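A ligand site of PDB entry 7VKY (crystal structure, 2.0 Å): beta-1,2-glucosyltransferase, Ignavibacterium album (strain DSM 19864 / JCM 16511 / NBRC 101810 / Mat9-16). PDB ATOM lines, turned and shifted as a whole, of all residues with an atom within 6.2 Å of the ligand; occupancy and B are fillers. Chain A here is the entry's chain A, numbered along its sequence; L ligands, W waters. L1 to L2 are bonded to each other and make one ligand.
O5 of LG2 L2 lies within hydrogen-bond range of OE1 of Glu 97 (2.5 Å). The side-chain hydroxyl of Tyr 373 lies within hydrogen-bond range of an oxygen (O3) of LG2 L2 (2.6 Å). The side-chain carboxylate of Glu 338 is in hydrogen-bond range of an oxygen (O1) of LG2 L2, at 2.7 Å. An oxygen (O3) of LIG L1 sits at hydrogen-bond distance from the side-chain carboxylate (OE2) of Glu 171, at 2.7 Å. An oxygen (O4) of LIG L1 sits at hydrogen-bond distance from the backbone NH (N) of Trp 274. O of Trp 274 is in hydrogen-bond range of O6 of LIG L1 (2.7 Å). The side-chain amide nitrogen (ND2) of Asn 170 is in hydrogen-bond range of an oxygen (O1) of LG2 L2 (2.8 Å). O2 of LG2 L2 lies within hydrogen-bond range of OH of Tyr 47, 2.8 Å away. N of Ala 96 sits at hydrogen-bond distance from O2 of LG2 L2, at 2.8 Å. The guanidinium group (NH1) of Arg 344 lies within hydrogen-bond range of an oxygen (O6) of LIG L1 (2.8 Å). O of Ile 94 is in hydrogen-bond range of O2 of LG2 L2 (2.9 Å). N of Gly 273 sits at hydrogen-bond distance from O4 of LIG L1 (3.0 Å).
The side-chain carboxylate of Glu 338 is in hydrogen-bond range of the side-chain hydroxyl of Tyr 47. N of Glu 171 sits at hydrogen-bond distance from OD1 of Asn 270. The side-chain carboxylate (OD2) of Asp 304 lies close to the side-chain carboxylate (OE2) of Glu 171, at 2.6 Å. OD1 of Asn 170 sits at hydrogen-bond distance from OH of Tyr 47 (2.7 Å). The side-chain amide oxygen of Asn 170 lies within hydrogen-bond range of the side-chain amide nitrogen of Gln 167 (2.9 Å). The side-chain hydroxyl (OH) of Tyr 47 lies within hydrogen-bond range of the backbone carbonyl oxygen (O) of Ile 94. OD2 of Asp 304 lies within hydrogen-bond range of ND2 of Asn 270, at 3.2 Å. The side-chain amide oxygen (OD1) of Asn 270 is in hydrogen-bond range of the side-chain amide nitrogen (NE2) of Gln 167 (3.2 Å).
Residues that only touch the ligand: Tyr 392 (3.3 Å), Trp 177 (3.5 Å), Leu 95 (3.5 Å), Asn 270 (3.5 Å), Pro 272 (3.8 Å), Ile 275 (3.8 Å), Ile 306 (3.8 Å) and Leu 178 (3.97 Å). Hydrophobic or aromatic side chains that line the ligand: Tyr 47, Leu 95, Ala 96, Trp 177, Leu 178, Ile 275, Ile 306 and Tyr 373. Of the 30 residues printed, 19 come within 4 Å of the ligand. Along chain A the residues within 4 Å of the ligand span positions 47 to 392.
Water W2 lies within hydrogen-bond range of the backbone carbonyl oxygen (O) of Asp 304 (2.6 Å), an oxygen (O3) of LIG L1 (2.8 Å), the backbone NH (N) of Trp 274 (2.9 Å) and the backbone NH (N) of Gly 273 (3.3 Å). Water W1 bridges the side-chain carboxylate of Glu 338 and an oxygen (O4) of LG2 L2.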
ATOM      1  N   HIS A  20       0.438  18.908  14.643  1.00  0.00           N
ATOM      2  CA  HIS A  20       1.905  19.111  14.807  1.00  0.00           C
ATOM      3  C   HIS A  20       2.132  20.376  15.643  1.00  0.00           C
ATOM      4  O   HIS A  20       2.077  21.481  15.058  1.00  0.00           O
ATOM      5  CB  HIS A  20       2.609  19.126  13.443  1.00  0.00           C
ATOM      6  CG  HIS A  20       2.685  17.793  12.791  1.00  0.00           C
ATOM      7  ND1 HIS A  20       3.168  17.636  11.516  1.00  0.00           N
ATOM      8  CD2 HIS A  20       2.369  16.566  13.247  1.00  0.00           C
ATOM      9  CE1 HIS A  20       3.136  16.383  11.180  1.00  0.00           C
ATOM     10  NE2 HIS A  20       2.628  15.693  12.221  1.00  0.00           N
ATOM     11  N   TYR A  47       4.472  13.891  15.527  1.00  0.00           N
ATOM     12  CA  TYR A  47       5.925  13.703  15.510  1.00  0.00           C
ATOM     13  C   TYR A  47       6.548  14.569  16.604  1.00  0.00           C
ATOM     14  O   TYR A  47       6.011  15.592  16.993  1.00  0.00           O
ATOM     15  CB  TYR A  47       6.458  14.032  14.114  1.00  0.00           C
ATOM     16  CG  TYR A  47       6.042  13.080  13.025  1.00  0.00           C
ATOM     17  CD1 TYR A  47       6.474  11.771  12.994  1.00  0.00           C
ATOM     18  CD2 TYR A  47       5.263  13.515  11.963  1.00  0.00           C
ATOM     19  CE1 TYR A  47       6.159  10.926  11.939  1.00  0.00           C
ATOM     20  CE2 TYR A  47       4.876  12.669  10.949  1.00  0.00           C
ATOM     21  CZ  TYR A  47       5.352  11.384  10.913  1.00  0.00           C
ATOM     22  OH  TYR A  47       5.001  10.611   9.839  1.00  0.00           O
ATOM     23  N   ILE A  94      11.175  11.143  10.509  1.00  0.00           N
ATOM     24  CA  ILE A  94       9.707  11.437  10.537  1.00  0.00           C
ATOM     25  C   ILE A  94       9.149  11.661   9.134  1.00  0.00           C
ATOM     26  O   ILE A  94       7.907  11.474   8.930  1.00  0.00           O
ATOM     27  CB  ILE A  94       9.426  12.631  11.469  1.00  0.00           C
ATOM     28  CG1 ILE A  94       9.999  13.937  10.933  1.00  0.00           C
ATOM     29  CG2 ILE A  94       9.923  12.325  12.875  1.00  0.00           C
ATOM     30  CD1 ILE A  94       9.450  15.171  11.634  1.00  0.00           C
ATOM     31  N   LEU A  95      10.010  12.040   8.191  1.00  0.00           N
ATOM     32  CA  LEU A  95       9.614  12.496   6.834  1.00  0.00           C
ATOM     33  C   LEU A  95       8.773  13.764   7.001  1.00  0.00           C
ATOM     34  O   LEU A  95       9.374  14.815   7.231  1.00  0.00           O
ATOM     35  CB  LEU A  95       8.901  11.359   6.076  1.00  0.00           C
ATOM     36  CG  LEU A  95       8.967  11.434   4.543  1.00  0.00           C
ATOM     37  CD1 LEU A  95       8.440  10.142   3.919  1.00  0.00           C
ATOM     38  CD2 LEU A  95       8.194  12.623   3.985  1.00  0.00           C
ATOM     39  N   ALA A  96       7.434  13.654   6.998  1.00  0.00           N
ATOM     40  CA  ALA A  96       6.498  14.709   7.445  1.00  0.00           C
ATOM     41  C   ALA A  96       6.676  16.016   6.631  1.00  0.00           C
ATOM     42  O   ALA A  96       6.363  17.098   7.175  1.00  0.00           O
ATOM     43  CB  ALA A  96       6.708  14.958   8.914  1.00  0.00           C
ATOM     44  N   GLU A  97       7.185  15.968   5.401  1.00  0.00           N
ATOM     45  CA  GLU A  97       7.498  17.178   4.600  1.00  0.00           C
ATOM     46  C   GLU A  97       8.349  18.149   5.437  1.00  0.00           C
ATOM     47  O   GLU A  97       8.160  19.390   5.317  1.00  0.00           O
ATOM     48  CB  GLU A  97       6.204  17.838   4.074  1.00  0.00           C
ATOM     49  CG  GLU A  97       5.550  17.031   2.959  1.00  0.00           C
ATOM     50  CD  GLU A  97       4.934  15.724   3.450  1.00  0.00           C
ATOM     51  OE1 GLU A  97       5.116  14.717   2.789  1.00  0.00           O
ATOM     52  OE2 GLU A  97       4.271  15.704   4.494  1.00  0.00           O
ATOM     53  N   GLN A 167       5.307   5.521  17.898  1.00  0.00           N
ATOM     54  CA  GLN A 167       5.785   5.001  16.605  1.00  0.00           C
ATOM     55  C   GLN A 167       7.315   4.944  16.618  1.00  0.00           C
ATOM     56  O   GLN A 167       7.964   5.937  17.019  1.00  0.00           O
ATOM     57  CB  GLN A 167       5.274   5.874  15.458  1.00  0.00           C
ATOM     58  CG  GLN A 167       5.480   5.285  14.077  1.00  0.00           C
ATOM     59  CD  GLN A 167       4.951   6.187  12.996  1.00  0.00           C
ATOM     60  OE1 GLN A 167       3.757   6.212  12.700  1.00  0.00           O
ATOM     61  NE2 GLN A 167       5.846   6.945  12.382  1.00  0.00           N
ATOM     62  N   ASN A 170       9.854   5.878  11.055  1.00  0.00           N
ATOM     63  CA  ASN A 170       8.762   6.237  10.133  1.00  0.00           C
ATOM     64  C   ASN A 170       8.943   5.470   8.832  1.00  0.00           C
ATOM     65  O   ASN A 170       9.962   5.706   8.150  1.00  0.00           O
ATOM     66  CB  ASN A 170       8.737   7.734   9.878  1.00  0.00           C
ATOM     67  CG  ASN A 170       7.431   8.168   9.256  1.00  0.00           C
ATOM     68  OD1 ASN A 170       6.410   8.332   9.939  1.00  0.00           O
ATOM     69  ND2 ASN A 170       7.454   8.371   7.962  1.00  0.00           N
ATOM     70  N   GLU A 171       8.002   4.625   8.474  1.00  0.00           N
ATOM     71  CA  GLU A 171       7.959   3.942   7.140  1.00  0.00           C
ATOM     72  C   GLU A 171       9.358   3.475   6.735  1.00  0.00           C
ATOM     73  O   GLU A 171       9.951   3.959   5.706  1.00  0.00           O
ATOM     74  CB  GLU A 171       7.371   4.894   6.102  1.00  0.00           C
ATOM     75  CG  GLU A 171       5.969   5.385   6.419  1.00  0.00           C
ATOM     76  CD  GLU A 171       5.448   6.274   5.296  1.00  0.00           C
ATOM     77  OE1 GLU A 171       6.292   7.011   4.697  1.00  0.00           O
ATOM     78  OE2 GLU A 171       4.213   6.207   5.009  1.00  0.00           O
ATOM     79  N   VAL A 174      11.035   3.577   3.184  1.00  0.00           N
ATOM     80  CA  VAL A 174      10.297   4.521   2.267  1.00  0.00           C
ATOM     81  C   VAL A 174      11.314   5.399   1.514  1.00  0.00           C
ATOM     82  O   VAL A 174      11.117   5.616   0.333  1.00  0.00           O
ATOM     83  CB  VAL A 174       9.267   5.418   2.979  1.00  0.00           C
ATOM     84  CG1 VAL A 174       9.903   6.479   3.883  1.00  0.00           C
ATOM     85  CG2 VAL A 174       8.338   6.067   1.955  1.00  0.00           C
ATOM     86  N   TRP A 177      13.184   3.443  -1.120  1.00  0.00           N
ATOM     87  CA  TRP A 177      12.198   3.179  -2.197  1.00  0.00           C
ATOM     88  C   TRP A 177      12.047   4.432  -3.081  1.00  0.00           C
ATOM     89  O   TRP A 177      12.173   4.331  -4.312  1.00  0.00           O
ATOM     90  CB  TRP A 177      10.877   2.722  -1.560  1.00  0.00           C
ATOM     91  CG  TRP A 177       9.700   2.634  -2.475  1.00  0.00           C
ATOM     92  CD1 TRP A 177       9.537   1.784  -3.541  1.00  0.00           C
ATOM     93  CD2 TRP A 177       8.457   3.341  -2.336  1.00  0.00           C
ATOM     94  NE1 TRP A 177       8.280   1.951  -4.070  1.00  0.00           N
ATOM     95  CE2 TRP A 177       7.587   2.866  -3.334  1.00  0.00           C
ATOM     96  CE3 TRP A 177       7.982   4.306  -1.444  1.00  0.00           C
ATOM     97  CZ2 TRP A 177       6.304   3.373  -3.519  1.00  0.00           C
ATOM     98  CZ3 TRP A 177       6.713   4.806  -1.601  1.00  0.00           C
ATOM     99  CH2 TRP A 177       5.890   4.343  -2.615  1.00  0.00           C
ATOM    100  N   LEU A 178      11.760   5.600  -2.494  1.00  0.00           N
ATOM    101  CA  LEU A 178      11.532   6.844  -3.286  1.00  0.00           C
ATOM    102  C   LEU A 178      12.813   7.277  -4.021  1.00  0.00           C
ATOM    103  O   LEU A 178      12.685   7.814  -5.085  1.00  0.00           O
ATOM    104  CB  LEU A 178      11.027   7.945  -2.360  1.00  0.00           C
ATOM    105  CG  LEU A 178       9.616   7.752  -1.791  1.00  0.00           C
ATOM    106  CD1 LEU A 178       9.383   8.845  -0.761  1.00  0.00           C
ATOM    107  CD2 LEU A 178       8.551   7.780  -2.885  1.00  0.00           C
ATOM    108  N   ASN A 270       4.367   2.288  10.688  1.00  0.00           N
ATOM    109  CA  ASN A 270       3.442   2.824   9.665  1.00  0.00           C
ATOM    110  C   ASN A 270       3.935   2.398   8.276  1.00  0.00           C
ATOM    111  O   ASN A 270       5.137   2.509   8.014  1.00  0.00           O
ATOM    112  CB  ASN A 270       3.292   4.330   9.824  1.00  0.00           C
ATOM    113  CG  ASN A 270       4.608   5.070   9.797  1.00  0.00           C
ATOM    114  OD1 ASN A 270       5.635   4.559  10.251  1.00  0.00           O
ATOM    115  ND2 ASN A 270       4.549   6.319   9.376  1.00  0.00           N
ATOM    116  N   ILE A 271       2.989   1.957   7.453  1.00  0.00           N
ATOM    117  CA  ILE A 271       3.197   1.300   6.137  1.00  0.00           C
ATOM    118  C   ILE A 271       3.038   2.316   5.013  1.00  0.00           C
ATOM    119  O   ILE A 271       1.936   2.849   4.774  1.00  0.00           O
ATOM    120  CB  ILE A 271       2.248   0.113   5.945  1.00  0.00           C
ATOM    121  CG1 ILE A 271       2.346  -0.897   7.089  1.00  0.00           C
ATOM    122  CG2 ILE A 271       2.526  -0.522   4.591  1.00  0.00           C
ATOM    123  CD1 ILE A 271       1.142  -1.802   7.238  1.00  0.00           C
ATOM    124  N   PRO A 272       4.112   2.527   4.209  1.00  0.00           N
ATOM    125  CA  PRO A 272       4.038   3.371   3.009  1.00  0.00           C
ATOM    126  C   PRO A 272       3.522   2.567   1.784  1.00  0.00           C
ATOM    127  O   PRO A 272       3.434   1.325   1.862  1.00  0.00           O
ATOM    128  CB  PRO A 272       5.514   3.773   2.823  1.00  0.00           C
ATOM    129  CG  PRO A 272       6.258   2.511   3.227  1.00  0.00           C
ATOM    130  CD  PRO A 272       5.449   1.928   4.369  1.00  0.00           C
ATOM    131  N   GLY A 273       3.221   3.275   0.676  1.00  0.00           N
ATOM    132  CA  GLY A 273       2.986   2.593  -0.610  1.00  0.00           C
ATOM    133  C   GLY A 273       2.030   3.309  -1.524  1.00  0.00           C
ATOM    134  O   GLY A 273       2.051   3.003  -2.736  1.00  0.00           O
ATOM    135  N   TRP A 274       1.170   4.194  -1.019  1.00  0.00           N
ATOM    136  CA  TRP A 274       0.272   4.937  -1.929  1.00  0.00           C
ATOM    137  C   TRP A 274       1.118   5.974  -2.676  1.00  0.00           C
ATOM    138  O   TRP A 274       2.004   6.599  -2.044  1.00  0.00           O
ATOM    139  CB  TRP A 274      -0.870   5.644  -1.216  1.00  0.00           C
ATOM    140  CG  TRP A 274      -1.939   4.771  -0.648  1.00  0.00           C
ATOM    141  CD1 TRP A 274      -1.842   4.005   0.474  1.00  0.00           C
ATOM    142  CD2 TRP A 274      -3.272   4.620  -1.140  1.00  0.00           C
ATOM    143  NE1 TRP A 274      -3.041   3.362   0.715  1.00  0.00           N
ATOM    144  CE2 TRP A 274      -3.948   3.745  -0.242  1.00  0.00           C
ATOM    145  CE3 TRP A 274      -3.979   5.131  -2.246  1.00  0.00           C
ATOM    146  CZ2 TRP A 274      -5.281   3.380  -0.417  1.00  0.00           C
ATOM    147  CZ3 TRP A 274      -5.300   4.782  -2.401  1.00  0.00           C
ATOM    148  CH2 TRP A 274      -5.944   3.926  -1.496  1.00  0.00           C
ATOM    149  N   ILE A 275       0.840   6.130  -3.962  1.00  0.00           N
ATOM    150  CA  ILE A 275       1.471   7.191  -4.789  1.00  0.00           C
ATOM    151  C   ILE A 275       0.491   7.489  -5.924  1.00  0.00           C
ATOM    152  O   ILE A 275      -0.105   6.560  -6.449  1.00  0.00           O
ATOM    153  CB  ILE A 275       2.888   6.794  -5.273  1.00  0.00           C
ATOM    154  CG1 ILE A 275       3.604   8.044  -5.803  1.00  0.00           C
ATOM    155  CG2 ILE A 275       2.877   5.650  -6.282  1.00  0.00           C
ATOM    156  CD1 ILE A 275       5.104   7.903  -5.995  1.00  0.00           C
ATOM    157  N   TYR A 276       0.238   8.761  -6.174  1.00  0.00           N
ATOM    158  CA  TYR A 276      -0.678   9.238  -7.243  1.00  0.00           C
ATOM    159  C   TYR A 276      -2.076   8.678  -7.019  1.00  0.00           C
ATOM    160  O   TYR A 276      -2.845   8.642  -7.977  1.00  0.00           O
ATOM    161  CB  TYR A 276      -0.135   8.899  -8.643  1.00  0.00           C
ATOM    162  CG  TYR A 276       1.310   9.271  -8.858  1.00  0.00           C
ATOM    163  CD1 TYR A 276       1.758  10.549  -8.579  1.00  0.00           C
ATOM    164  CD2 TYR A 276       2.244   8.361  -9.324  1.00  0.00           C
ATOM    165  CE1 TYR A 276       3.086  10.908  -8.728  1.00  0.00           C
ATOM    166  CE2 TYR A 276       3.581   8.705  -9.506  1.00  0.00           C
ATOM    167  CZ  TYR A 276       4.011   9.980  -9.194  1.00  0.00           C
ATOM    168  OH  TYR A 276       5.320  10.349  -9.350  1.00  0.00           O
ATOM    169  N   LEU A 285       6.008  -3.135  -0.338  1.00  0.00           N
ATOM    170  CA  LEU A 285       6.619  -2.463   0.824  1.00  0.00           C
ATOM    171  C   LEU A 285       6.218  -3.184   2.111  1.00  0.00           C
ATOM    172  O   LEU A 285       7.114  -3.428   2.948  1.00  0.00           O
ATOM    173  CB  LEU A 285       6.218  -0.980   0.824  1.00  0.00           C
ATOM    174  CG  LEU A 285       6.775  -0.223  -0.371  1.00  0.00           C
ATOM    175  CD1 LEU A 285       6.256   1.216  -0.419  1.00  0.00           C
ATOM    176  CD2 LEU A 285       8.282  -0.249  -0.322  1.00  0.00           C
ATOM    177  N   ASP A 304      -0.855   3.721   5.904  1.00  0.00           N
ATOM    178  CA  ASP A 304      -0.823   5.157   5.566  1.00  0.00           C
ATOM    179  C   ASP A 304      -1.583   5.320   4.257  1.00  0.00           C
ATOM    180  O   ASP A 304      -0.999   5.080   3.204  1.00  0.00           O
ATOM    181  CB  ASP A 304       0.613   5.663   5.575  1.00  0.00           C
ATOM    182  CG  ASP A 304       1.292   5.549   6.929  1.00  0.00           C
ATOM    183  OD1 ASP A 304       0.591   5.403   7.968  1.00  0.00           O
ATOM    184  OD2 ASP A 304       2.545   5.644   6.932  1.00  0.00           O
ATOM    185  N   ILE A 306      -3.387   7.310   1.314  1.00  0.00           N
ATOM    186  CA  ILE A 306      -3.370   8.604   0.572  1.00  0.00           C
ATOM    187  C   ILE A 306      -4.091   8.406  -0.760  1.00  0.00           C
ATOM    188  O   ILE A 306      -3.476   8.427  -1.828  1.00  0.00           O
ATOM    189  CB  ILE A 306      -1.946   9.096   0.359  1.00  0.00           C
ATOM    190  CG1 ILE A 306      -1.066   8.888   1.586  1.00  0.00           C
ATOM    191  CG2 ILE A 306      -1.954  10.543  -0.105  1.00  0.00           C
ATOM    192  CD1 ILE A 306       0.367   9.256   1.311  1.00  0.00           C
ATOM    193  N   GLU A 308      -6.154  10.547  -2.409  1.00  0.00           N
ATOM    194  CA  GLU A 308      -6.095  11.811  -3.211  1.00  0.00           C
ATOM    195  C   GLU A 308      -7.436  12.141  -3.887  1.00  0.00           C
ATOM    196  O   GLU A 308      -7.752  13.342  -4.053  1.00  0.00           O
ATOM    197  CB  GLU A 308      -5.024  11.761  -4.297  1.00  0.00           C
ATOM    198  CG  GLU A 308      -3.646  11.547  -3.718  1.00  0.00           C
ATOM    199  CD  GLU A 308      -2.476  11.681  -4.663  1.00  0.00           C
ATOM    200  OE1 GLU A 308      -2.711  11.850  -5.872  1.00  0.00           O
ATOM    201  OE2 GLU A 308      -1.342  11.605  -4.190  1.00  0.00           O
ATOM    202  N   GLU A 338      -1.896   6.814   9.320  1.00  0.00           N
ATOM    203  CA  GLU A 338      -2.046   8.087   8.580  1.00  0.00           C
ATOM    204  C   GLU A 338      -3.240   7.920   7.651  1.00  0.00           C
ATOM    205  O   GLU A 338      -3.193   7.079   6.738  1.00  0.00           O
ATOM    206  CB  GLU A 338      -0.784   8.452   7.792  1.00  0.00           C
ATOM    207  CG  GLU A 338       0.439   8.673   8.680  1.00  0.00           C
ATOM    208  CD  GLU A 338       1.745   8.829   7.931  1.00  0.00           C
ATOM    209  OE1 GLU A 338       1.689   9.091   6.673  1.00  0.00           O
ATOM    210  OE2 GLU A 338       2.814   8.627   8.565  1.00  0.00           O
ATOM    211  N   ARG A 344      -1.112  16.984   1.291  1.00  0.00           N
ATOM    212  CA  ARG A 344       0.302  17.320   1.564  1.00  0.00           C
ATOM    213  C   ARG A 344       0.858  18.319   0.540  1.00  0.00           C
ATOM    214  O   ARG A 344       1.943  18.877   0.826  1.00  0.00           O
ATOM    215  CB  ARG A 344       1.149  16.049   1.497  1.00  0.00           C
ATOM    216  CG  ARG A 344       1.137  15.374   0.130  1.00  0.00           C
ATOM    217  CD  ARG A 344       1.732  13.986   0.282  1.00  0.00           C
ATOM    218  NE  ARG A 344       1.615  13.192  -0.928  1.00  0.00           N
ATOM    219  CZ  ARG A 344       2.282  12.063  -1.120  1.00  0.00           C
ATOM    220  NH1 ARG A 344       2.166  11.412  -2.259  1.00  0.00           N
ATOM    221  NH2 ARG A 344       3.039  11.573  -0.161  1.00  0.00           N
ATOM    222  N   TYR A 373      -4.784  12.489   9.126  1.00  0.00           N
ATOM    223  CA  TYR A 373      -3.450  13.036   8.768  1.00  0.00           C
ATOM    224  C   TYR A 373      -3.614  13.880   7.500  1.00  0.00           C
ATOM    225  O   TYR A 373      -3.663  13.296   6.438  1.00  0.00           O
ATOM    226  CB  TYR A 373      -2.440  11.887   8.607  1.00  0.00           C
ATOM    227  CG  TYR A 373      -0.997  12.336   8.550  1.00  0.00           C
ATOM    228  CD1 TYR A 373      -0.489  12.928   7.390  1.00  0.00           C
ATOM    229  CD2 TYR A 373      -0.178  12.236   9.652  1.00  0.00           C
ATOM    230  CE1 TYR A 373       0.804  13.392   7.335  1.00  0.00           C
ATOM    231  CE2 TYR A 373       1.144  12.686   9.602  1.00  0.00           C
ATOM    232  CZ  TYR A 373       1.634  13.264   8.444  1.00  0.00           C
ATOM    233  OH  TYR A 373       2.904  13.728   8.382  1.00  0.00           O
ATOM    234  N   MET A 374      -3.719  15.221   7.589  1.00  0.00           N
ATOM    235  CA  MET A 374      -3.557  16.016   8.792  1.00  0.00           C
ATOM    236  C   MET A 374      -4.912  16.549   9.268  1.00  0.00           C
ATOM    237  O   MET A 374      -5.636  17.165   8.476  1.00  0.00           O
ATOM    238  CB  MET A 374      -2.650  17.217   8.525  1.00  0.00           C
ATOM    239  CG  MET A 374      -1.189  16.874   8.272  1.00  0.00           C
ATOM    240  SD  MET A 374      -0.387  16.060   9.646  1.00  0.00           S
ATOM    241  CE  MET A 374      -0.587  17.356  10.889  1.00  0.00           C
ATOM    242  N   PHE A 391       2.312  23.611   5.711  1.00  0.00           N
ATOM    243  CA  PHE A 391       2.253  22.144   5.919  1.00  0.00           C
ATOM    244  C   PHE A 391       0.776  21.735   5.862  1.00  0.00           C
ATOM    245  O   PHE A 391       0.008  21.920   6.846  1.00  0.00           O
ATOM    246  CB  PHE A 391       2.942  21.672   7.203  1.00  0.00           C
ATOM    247  CG  PHE A 391       2.831  20.174   7.385  1.00  0.00           C
ATOM    248  CD1 PHE A 391       3.476  19.306   6.508  1.00  0.00           C
ATOM    249  CD2 PHE A 391       2.093  19.637   8.430  1.00  0.00           C
ATOM    250  CE1 PHE A 391       3.332  17.934   6.674  1.00  0.00           C
ATOM    251  CE2 PHE A 391       2.011  18.269   8.619  1.00  0.00           C
ATOM    252  CZ  PHE A 391       2.607  17.424   7.719  1.00  0.00           C
ATOM    253  N   TYR A 392       0.443  21.175   4.711  1.00  0.00           N
ATOM    254  CA  TYR A 392      -0.878  20.619   4.347  1.00  0.00           C
ATOM    255  C   TYR A 392      -1.878  21.747   4.049  1.00  0.00           C
ATOM    256  O   TYR A 392      -1.721  22.928   4.463  1.00  0.00           O
ATOM    257  CB  TYR A 392      -1.407  19.641   5.399  1.00  0.00           C
ATOM    258  CG  TYR A 392      -1.121  18.205   5.074  1.00  0.00           C
ATOM    259  CD1 TYR A 392       0.170  17.695   5.187  1.00  0.00           C
ATOM    260  CD2 TYR A 392      -2.128  17.301   4.751  1.00  0.00           C
ATOM    261  CE1 TYR A 392       0.459  16.368   4.901  1.00  0.00           C
ATOM    262  CE2 TYR A 392      -1.848  15.967   4.496  1.00  0.00           C
ATOM    263  CZ  TYR A 392      -0.551  15.488   4.560  1.00  0.00           C
ATOM    264  OH  TYR A 392      -0.229  14.190   4.261  1.00  0.00           O
ATOM    265  N   LEU A 451       9.073   2.349  -8.658  1.00  0.00           N
ATOM    266  CA  LEU A 451       9.983   3.464  -8.305  1.00  0.00           C
ATOM    267  C   LEU A 451      11.453   3.139  -8.618  1.00  0.00           C
ATOM    268  O   LEU A 451      12.250   4.069  -8.668  1.00  0.00           O
ATOM    269  CB  LEU A 451       9.734   3.830  -6.833  1.00  0.00           C
ATOM    270  CG  LEU A 451       8.575   4.816  -6.704  1.00  0.00           C
ATOM    271  CD1 LEU A 451       7.224   4.138  -6.789  1.00  0.00           C
ATOM    272  CD2 LEU A 451       8.672   5.630  -5.470  1.00  0.00           C
HETATM  273  C1  LIG L   1       4.455   8.976   2.263  1.00  0.00           C
HETATM  274  C2  LIG L   1       4.191   7.513   1.872  1.00  0.00           C
HETATM  275  C3  LIG L   1       3.921   7.481   0.368  1.00  0.00           C
HETATM  276  C4  LIG L   1       5.033   8.193  -0.412  1.00  0.00           C
HETATM  277  C5  LIG L   1       4.734   8.285  -1.902  1.00  0.00           C
HETATM  278  C6  LIG L   1       5.583   9.560   1.400  1.00  0.00           C
HETATM  279  O1  LIG L   1       5.753  10.936   1.747  1.00  0.00           O
HETATM  280  O2  LIG L   1       4.877   9.027   3.625  1.00  0.00           O
HETATM  281  O3  LIG L   1       3.109   6.997   2.684  1.00  0.00           O
HETATM  282  O4  LIG L   1       3.812   6.134  -0.086  1.00  0.00           O
HETATM  283  O5  LIG L   1       5.198   9.547   0.025  1.00  0.00           O
HETATM  284  O6  LIG L   1       3.440   8.874  -2.048  1.00  0.00           O
HETATM  285  C1  LG2 L   2       4.764   9.894   5.927  1.00  0.00           C
HETATM  286  C2  LG2 L   2       4.326  11.233   6.539  1.00  0.00           C
HETATM  287  C3  LG2 L   2       3.992  12.264   5.461  1.00  0.00           C
HETATM  288  C4  LG2 L   2       2.836  11.713   4.629  1.00  0.00           C
HETATM  289  C5  LG2 L   2       2.531  12.557   3.390  1.00  0.00           C
HETATM  290  C6  LG2 L   2       3.941   9.389   4.707  1.00  0.00           C
HETATM  291  O1  LG2 L   2       4.920   8.902   6.972  1.00  0.00           O
HETATM  292  O2  LG2 L   2       5.458  11.663   7.304  1.00  0.00           O
HETATM  293  O3  LG2 L   2       3.744  13.603   5.945  1.00  0.00           O
HETATM  294  O4  LG2 L   2       2.967  10.319   4.198  1.00  0.00           O
HETATM  295  O5  LG2 L   2       3.629  12.680   2.445  1.00  0.00           O
HETATM  296  O   HOH W   1       0.127   9.329   4.744  1.00  0.00           O
HETATM  297  O   HOH W   2       1.023   5.549   1.568  1.00  0.00           O
